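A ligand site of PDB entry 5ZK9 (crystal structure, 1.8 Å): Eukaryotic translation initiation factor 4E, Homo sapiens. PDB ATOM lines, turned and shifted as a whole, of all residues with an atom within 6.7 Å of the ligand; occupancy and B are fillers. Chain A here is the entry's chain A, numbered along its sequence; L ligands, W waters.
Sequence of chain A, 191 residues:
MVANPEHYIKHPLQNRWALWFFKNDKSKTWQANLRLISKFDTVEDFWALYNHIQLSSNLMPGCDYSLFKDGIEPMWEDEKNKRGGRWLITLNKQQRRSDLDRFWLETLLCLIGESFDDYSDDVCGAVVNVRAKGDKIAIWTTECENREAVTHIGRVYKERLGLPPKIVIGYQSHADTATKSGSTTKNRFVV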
ATOM      1  N   PHE A  22      28.582 -16.496  18.943  1.00  0.00           N
ATOM      2  CA  PHE A  22      27.373 -15.692  18.895  1.00  0.00           C
ATOM      3  C   PHE A  22      26.178 -16.631  18.946  1.00  0.00           C
ATOM      4  O   PHE A  22      26.147 -17.632  18.245  1.00  0.00           O
ATOM      5  CB  PHE A  22      27.323 -14.866  17.607  1.00  0.00           C
ATOM      6  CG  PHE A  22      26.086 -14.001  17.494  1.00  0.00           C
ATOM      7  CD1 PHE A  22      24.885 -14.545  17.020  1.00  0.00           C
ATOM      8  CD2 PHE A  22      26.123 -12.665  17.838  1.00  0.00           C
ATOM      9  CE1 PHE A  22      23.739 -13.761  16.917  1.00  0.00           C
ATOM     10  CE2 PHE A  22      24.985 -11.877  17.717  1.00  0.00           C
ATOM     11  CZ  PHE A  22      23.806 -12.426  17.261  1.00  0.00           C
ATOM     12  N   TRP A  30      22.348  -6.647  19.000  1.00  0.00           N
ATOM     13  CA  TRP A  30      23.177  -7.701  18.382  1.00  0.00           C
ATOM     14  C   TRP A  30      24.470  -7.931  19.174  1.00  0.00           C
ATOM     15  O   TRP A  30      24.800  -9.063  19.536  1.00  0.00           O
ATOM     16  CB  TRP A  30      23.474  -7.338  16.908  1.00  0.00           C
ATOM     17  CG  TRP A  30      24.398  -8.302  16.194  1.00  0.00           C
ATOM     18  CD1 TRP A  30      24.049  -9.445  15.556  1.00  0.00           C
ATOM     19  CD2 TRP A  30      25.822  -8.177  16.058  1.00  0.00           C
ATOM     20  NE1 TRP A  30      25.165 -10.066  15.044  1.00  0.00           N
ATOM     21  CE2 TRP A  30      26.264  -9.305  15.324  1.00  0.00           C
ATOM     22  CE3 TRP A  30      26.767  -7.238  16.488  1.00  0.00           C
ATOM     23  CZ2 TRP A  30      27.609  -9.506  15.013  1.00  0.00           C
ATOM     24  CZ3 TRP A  30      28.099  -7.436  16.172  1.00  0.00           C
ATOM     25  CH2 TRP A  30      28.508  -8.565  15.447  1.00  0.00           C
ATOM     26  N   GLN A  31      25.213  -6.843  19.411  1.00  0.00           N
ATOM     27  CA  GLN A  31      26.564  -6.922  20.004  1.00  0.00           C
ATOM     28  C   GLN A  31      26.625  -7.625  21.388  1.00  0.00           C
ATOM     29  O   GLN A  31      27.624  -8.257  21.716  1.00  0.00           O
ATOM     30  CB  GLN A  31      27.169  -5.513  20.076  1.00  0.00           C
ATOM     31  CG  GLN A  31      28.502  -5.401  20.789  1.00  0.00           C
ATOM     32  CD  GLN A  31      29.016  -3.976  20.849  1.00  0.00           C
ATOM     33  OE1 GLN A  31      28.555  -3.106  20.107  1.00  0.00           O
ATOM     34  NE2 GLN A  31      29.961  -3.740  21.750  1.00  0.00           N
ATOM     35  N   GLY A  62      21.310 -20.030  13.721  1.00  0.00           N
ATOM     36  CA  GLY A  62      21.397 -18.702  14.314  1.00  0.00           C
ATOM     37  C   GLY A  62      22.679 -18.422  15.063  1.00  0.00           C
ATOM     38  O   GLY A  62      22.873 -17.303  15.557  1.00  0.00           O
ATOM     39  N   ASP A  64      26.991 -18.194  15.430  1.00  0.00           N
ATOM     40  CA  ASP A  64      28.217 -17.923  14.674  1.00  0.00           C
ATOM     41  C   ASP A  64      29.431 -18.303  15.502  1.00  0.00           C
ATOM     42  O   ASP A  64      29.428 -18.202  16.750  1.00  0.00           O
ATOM     43  CB  ASP A  64      28.430 -16.438  14.318  1.00  0.00           C
ATOM     44  CG  ASP A  64      27.203 -15.744  13.768  1.00  0.00           C
ATOM     45  OD1 ASP A  64      26.428 -16.352  13.025  1.00  0.00           O
ATOM     46  OD2 ASP A  64      27.067 -14.525  14.062  1.00  0.00           O
ATOM     47  N   PRO A  74      34.962  -8.672  16.312  1.00  0.00           N
ATOM     48  CA  PRO A  74      34.350  -9.291  15.127  1.00  0.00           C
ATOM     49  C   PRO A  74      33.086  -8.580  14.642  1.00  0.00           C
ATOM     50  O   PRO A  74      32.019  -9.198  14.492  1.00  0.00           O
ATOM     51  CB  PRO A  74      34.067 -10.728  15.607  1.00  0.00           C
ATOM     52  CG  PRO A  74      33.815 -10.582  17.071  1.00  0.00           C
ATOM     53  CD  PRO A  74      34.707  -9.465  17.528  1.00  0.00           C
ATOM     54  N   MET A  75      33.208  -7.284  14.376  1.00  0.00           N
ATOM     55  CA  MET A  75      32.075  -6.458  13.990  1.00  0.00           C
ATOM     56  C   MET A  75      32.517  -5.329  13.071  1.00  0.00           C
ATOM     57  O   MET A  75      33.686  -4.889  13.084  1.00  0.00           O
ATOM     58  CB  MET A  75      31.361  -5.909  15.231  1.00  0.00           C
ATOM     59  CG  MET A  75      32.239  -5.038  16.103  1.00  0.00           C
ATOM     60  SD  MET A  75      31.339  -4.445  17.552  1.00  0.00           S
ATOM     61  CE  MET A  75      31.432  -5.850  18.629  1.00  0.00           C
ATOM     62  N   TRP A  76      31.568  -4.880  12.255  1.00  0.00           N
ATOM     63  CA  TRP A  76      31.801  -3.866  11.218  1.00  0.00           C
ATOM     64  C   TRP A  76      32.449  -2.609  11.791  1.00  0.00           C
ATOM     65  O   TRP A  76      33.282  -1.972  11.149  1.00  0.00           O
ATOM     66  CB  TRP A  76      30.480  -3.438  10.554  1.00  0.00           C
ATOM     67  CG  TRP A  76      29.683  -4.537   9.931  1.00  0.00           C
ATOM     68  CD1 TRP A  76      30.161  -5.620   9.243  1.00  0.00           C
ATOM     69  CD2 TRP A  76      28.263  -4.651   9.917  1.00  0.00           C
ATOM     70  NE1 TRP A  76      29.121  -6.402   8.817  1.00  0.00           N
ATOM     71  CE2 TRP A  76      27.945  -5.816   9.210  1.00  0.00           C
ATOM     72  CE3 TRP A  76      27.216  -3.870  10.446  1.00  0.00           C
ATOM     73  CZ2 TRP A  76      26.607  -6.243   9.023  1.00  0.00           C
ATOM     74  CZ3 TRP A  76      25.908  -4.299  10.259  1.00  0.00           C
ATOM     75  CH2 TRP A  76      25.620  -5.466   9.553  1.00  0.00           C
ATOM     76  N   GLU A  77      32.027  -2.267  13.008  1.00  0.00           N
ATOM     77  CA  GLU A  77      32.373  -1.010  13.657  1.00  0.00           C
ATOM     78  C   GLU A  77      33.819  -0.903  14.108  1.00  0.00           C
ATOM     79  O   GLU A  77      34.281   0.197  14.365  1.00  0.00           O
ATOM     80  CB  GLU A  77      31.470  -0.780  14.877  1.00  0.00           C
ATOM     81  CG  GLU A  77      30.009  -0.489  14.535  1.00  0.00           C
ATOM     82  CD  GLU A  77      29.107  -1.710  14.470  1.00  0.00           C
ATOM     83  OE1 GLU A  77      27.876  -1.514  14.519  1.00  0.00           O
ATOM     84  OE2 GLU A  77      29.594  -2.863  14.342  1.00  0.00           O
ATOM     85  N   ARG A  86      34.347  -8.478   3.057  1.00  0.00           N
ATOM     86  CA  ARG A  86      34.504  -9.917   3.154  1.00  0.00           C
ATOM     87  C   ARG A  86      34.433 -10.663   1.820  1.00  0.00           C
ATOM     88  O   ARG A  86      33.671 -10.306   0.917  1.00  0.00           O
ATOM     89  CB  ARG A  86      33.457 -10.497   4.106  1.00  0.00           C
ATOM     90  CG  ARG A  86      32.048 -10.368   3.565  1.00  0.00           C
ATOM     91  CD  ARG A  86      31.019 -10.880   4.538  1.00  0.00           C
ATOM     92  NE  ARG A  86      29.677 -10.753   3.958  1.00  0.00           N
ATOM     93  CZ  ARG A  86      28.570 -11.206   4.528  1.00  0.00           C
ATOM     94  NH1 ARG A  86      27.404 -11.008   3.912  1.00  0.00           N
ATOM     95  NH2 ARG A  86      28.614 -11.845   5.698  1.00  0.00           N
ATOM     96  N   VAL A 127      34.408 -15.508   9.717  1.00  0.00           N
ATOM     97  CA  VAL A 127      33.129 -15.740  10.383  1.00  0.00           C
ATOM     98  C   VAL A 127      32.406 -16.903   9.700  1.00  0.00           C
ATOM     99  O   VAL A 127      32.331 -16.961   8.473  1.00  0.00           O
ATOM    100  CB  VAL A 127      32.208 -14.507  10.298  1.00  0.00           C
ATOM    101  CG1 VAL A 127      30.896 -14.764  10.979  1.00  0.00           C
ATOM    102  CG2 VAL A 127      32.880 -13.280  10.897  1.00  0.00           C
ATOM    103  N   ASN A 129      28.529 -18.426   9.780  1.00  0.00           N
ATOM    104  CA  ASN A 129      27.141 -18.248  10.201  1.00  0.00           C
ATOM    105  C   ASN A 129      26.412 -19.562   9.902  1.00  0.00           C
ATOM    106  O   ASN A 129      26.316 -19.949   8.752  1.00  0.00           O
ATOM    107  CB  ASN A 129      26.455 -17.154   9.392  1.00  0.00           C
ATOM    108  CG  ASN A 129      27.205 -15.817   9.397  1.00  0.00           C
ATOM    109  OD1 ASN A 129      27.588 -15.314   8.338  1.00  0.00           O
ATOM    110  ND2 ASN A 129      27.379 -15.238  10.574  1.00  0.00           N
ATOM    111  N   ARG A 131      22.929 -21.089   9.580  1.00  0.00           N
ATOM    112  CA  ARG A 131      21.644 -20.473   9.299  1.00  0.00           C
ATOM    113  C   ARG A 131      20.752 -21.466   8.582  1.00  0.00           C
ATOM    114  O   ARG A 131      21.208 -22.167   7.689  1.00  0.00           O
ATOM    115  CB  ARG A 131      21.803 -19.258   8.416  1.00  0.00           C
ATOM    116  CG  ARG A 131      22.541 -18.090   9.040  1.00  0.00           C
ATOM    117  CD  ARG A 131      21.740 -17.433  10.147  1.00  0.00           C
ATOM    118  NE  ARG A 131      22.447 -16.276  10.668  1.00  0.00           N
ATOM    119  CZ  ARG A 131      23.476 -16.325  11.523  1.00  0.00           C
ATOM    120  NH1 ARG A 131      23.925 -17.476  12.005  1.00  0.00           N
ATOM    121  NH2 ARG A 131      24.037 -15.196  11.914  1.00  0.00           N
ATOM    122  N   GLY A 134      20.724 -21.306   4.785  1.00  0.00           N
ATOM    123  CA  GLY A 134      21.982 -21.591   4.103  1.00  0.00           C
ATOM    124  C   GLY A 134      23.125 -20.990   4.917  1.00  0.00           C
ATOM    125  O   GLY A 134      23.098 -19.817   5.289  1.00  0.00           O
ATOM    126  N   LYS A 136      26.969 -19.622   5.845  1.00  0.00           N
ATOM    127  CA  LYS A 136      27.924 -18.736   5.193  1.00  0.00           C
ATOM    128  C   LYS A 136      29.254 -18.830   5.918  1.00  0.00           C
ATOM    129  O   LYS A 136      29.295 -19.005   7.128  1.00  0.00           O
ATOM    130  CB  LYS A 136      27.441 -17.284   5.220  1.00  0.00           C
ATOM    131  CG  LYS A 136      26.294 -17.006   4.277  1.00  0.00           C
ATOM    132  CD  LYS A 136      25.658 -15.657   4.572  1.00  0.00           C
ATOM    133  CE  LYS A 136      24.793 -15.678   5.799  1.00  0.00           C
ATOM    134  NZ  LYS A 136      24.159 -14.345   5.938  1.00  0.00           N
ATOM    135  N   TRP A 140      37.266 -11.759   6.358  1.00  0.00           N
ATOM    136  CA  TRP A 140      37.108 -10.309   6.471  1.00  0.00           C
ATOM    137  C   TRP A 140      38.505  -9.709   6.300  1.00  0.00           C
ATOM    138  O   TRP A 140      39.486 -10.194   6.914  1.00  0.00           O
ATOM    139  CB  TRP A 140      36.571  -9.924   7.848  1.00  0.00           C
ATOM    140  CG  TRP A 140      35.145 -10.207   8.071  1.00  0.00           C
ATOM    141  CD1 TRP A 140      34.401 -11.215   7.543  1.00  0.00           C
ATOM    142  CD2 TRP A 140      34.275  -9.467   8.926  1.00  0.00           C
ATOM    143  NE1 TRP A 140      33.093 -11.136   7.998  1.00  0.00           N
ATOM    144  CE2 TRP A 140      32.999 -10.087   8.867  1.00  0.00           C
ATOM    145  CE3 TRP A 140      34.440  -8.358   9.758  1.00  0.00           C
ATOM    146  CZ2 TRP A 140      31.906  -9.616   9.587  1.00  0.00           C
ATOM    147  CZ3 TRP A 140      33.340  -7.893  10.474  1.00  0.00           C
ATOM    148  CH2 TRP A 140      32.105  -8.509  10.388  1.00  0.00           C
ATOM    149  N   THR A 177      27.226  -3.993   2.776  1.00  0.00           N
ATOM    150  CA  THR A 177      26.462  -4.999   3.524  1.00  0.00           C
ATOM    151  C   THR A 177      25.527  -4.365   4.573  1.00  0.00           C
ATOM    152  O   THR A 177      24.349  -4.749   4.667  1.00  0.00           O
ATOM    153  CB  THR A 177      27.410  -6.001   4.216  1.00  0.00           C
ATOM    154  OG1 THR A 177      28.258  -6.608   3.226  1.00  0.00           O
ATOM    155  CG2 THR A 177      26.612  -7.074   4.948  1.00  0.00           C
HETATM  156  P1  LIG L   1      24.317 -11.854   9.958  1.00  0.00           P
HETATM  157  O1  LIG L   1      24.326 -12.638  11.227  1.00  0.00           O
HETATM  158  O2  LIG L   1      25.616 -11.481   9.273  1.00  0.00           O
HETATM  159  O3  LIG L   1      23.447 -12.549   8.785  1.00  0.00           O
HETATM  160  O4  LIG L   1      23.512 -10.470  10.169  1.00  0.00           O
HETATM  161  P2  LIG L   1      22.027 -13.332   8.744  1.00  0.00           P
HETATM  162  O5  LIG L   1      21.582 -13.744  10.126  1.00  0.00           O
HETATM  163  O6  LIG L   1      22.194 -14.441   7.738  1.00  0.00           O
HETATM  164  O7  LIG L   1      21.066 -12.224   8.068  1.00  0.00           O
HETATM  165  P3  LIG L   1      21.489 -11.165   6.886  1.00  0.00           P
HETATM  166  O8  LIG L   1      22.993 -11.228   6.667  1.00  0.00           O
HETATM  167  O9  LIG L   1      20.719 -11.657   5.663  1.00  0.00           O
HETATM  168  O10 LIG L   1      21.068  -9.809   7.444  1.00  0.00           O
HETATM  169  C1  LIG L   1      22.227 -10.398  10.742  1.00  0.00           C
HETATM  170  C2  LIG L   1      22.039  -9.047  11.426  1.00  0.00           C
HETATM  171  O11 LIG L   1      22.859  -9.009  12.587  1.00  0.00           O
HETATM  172  C3  LIG L   1      22.467  -7.827  10.619  1.00  0.00           C
HETATM  173  O12 LIG L   1      21.503  -7.421   9.645  1.00  0.00           O
HETATM  174  C4  LIG L   1      22.666  -6.827  11.728  1.00  0.00           C
HETATM  175  O13 LIG L   1      21.421  -6.299  12.201  1.00  0.00           O
HETATM  176  C5  LIG L   1      23.343  -7.694  12.788  1.00  0.00           C
HETATM  177  N1  LIG L   1      24.815  -7.596  12.633  1.00  0.00           N
HETATM  178  C6  LIG L   1      25.526  -8.686  11.950  1.00  0.00           C
HETATM  179  N2  LIG L   1      26.852  -8.110  12.064  1.00  0.00           N
HETATM  180  C7  LIG L   1      27.942  -8.931  11.446  1.00  0.00           C
HETATM  181  C8  LIG L   1      26.907  -6.922  12.670  1.00  0.00           C
HETATM  182  C9  LIG L   1      27.997  -6.010  12.988  1.00  0.00           C
HETATM  183  O14 LIG L   1      29.200  -6.246  12.678  1.00  0.00           O
HETATM  184  N3  LIG L   1      27.630  -4.882  13.642  1.00  0.00           N
HETATM  185  C10 LIG L   1      26.356  -4.610  13.975  1.00  0.00           C
HETATM  186  N4  LIG L   1      26.092  -3.440  14.613  1.00  0.00           N
HETATM  187  N5  LIG L   1      25.291  -5.420  13.709  1.00  0.00           N
HETATM  188  C11 LIG L   1      25.539  -6.578  13.056  1.00  0.00           C
HETATM  189  O   HOH W   1      22.254 -12.667  13.909  1.00  0.00           O
HETATM  190  O   HOH W   2      25.880  -9.355   7.555  1.00  0.00           O
HETATM  191  O   HOH W   3      19.140 -14.832  10.017  1.00  0.00           O
HETATM  192  O   HOH W   4      20.468 -16.180   6.709  1.00  0.00           O
HETATM  193  O   HOH W   5      26.509 -13.085   7.296  1.00  0.00           O
HETATM  194  O   HOH W   6      22.771  -4.394  14.705  1.00  0.00           O
HETATM  195  O   HOH W   7      23.425  -2.902  16.634  1.00  0.00           O
HETATM  196  O   HOH W   8      20.406 -13.388  12.326  1.00  0.00           O
HETATM  197  O   HOH W   9      25.051 -12.661  13.742  1.00  0.00           O
HETATM  198  O   HOH W  10      28.779 -11.557   9.215  1.00  0.00           O
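N4 of the ligand lies within hydrogen-bond range of OE1 of Glu 77 (2.6 Å). An oxygen (O6) of the ligand lies within salt-bridge range of the side-chain amino group (NZ) of Lys 136, 2.7 Å away. An oxygen (O1) of the ligand lies within salt-bridge range of the guanidinium group of Arg 131 (2.7 Å). N of Trp 76 sits at hydrogen-bond distance from O14 of the ligand (2.8 Å).
NH2 of Arg 131 lies within salt-bridge range of OD1 of Asp 64, 2.9 Å away. The backbone carbonyl oxygen (O) of Lys 136 is in hydrogen-bond range of the backbone NH (N) of Asn 129 (2.8 Å).
The indole nitrogen (NE1) of Trp 30 lies close to a nitrogen (N1) of the ligand, 3.5 Å away. CA of Met 75 touches O14 of the ligand (3.2 Å). Hydrophobic or aromatic side chains within 4 Å of the ligand: Trp 30, Met 75 and Trp 76. Within 4 Å of the ligand: Trp 30, Met 75, Trp 76, Glu 77, Arg 131 and Lys 136. The nearest printed residue that does not touch the ligand is Asn 129 (4.1 Å).
Water W9 lies within hydrogen-bond range of an oxygen (O1) of the ligand (2.6 Å), the side-chain carboxylate of Asp 64 (2.8 Å), the indole nitrogen of Trp 30 (2.9 Å) and the guanidinium group of Arg 131 (3.3 Å). Water W5 lies within hydrogen-bond range of the side-chain amide oxygen (OD1) of Asn 129 (2.7 Å), an oxygen (O2) of the ligand (2.7 Å), the guanidinium group (NH2) of Arg 86 (2.9 Å) and the side-chain amino group (NZ) of Lys 136 (3.0 Å).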
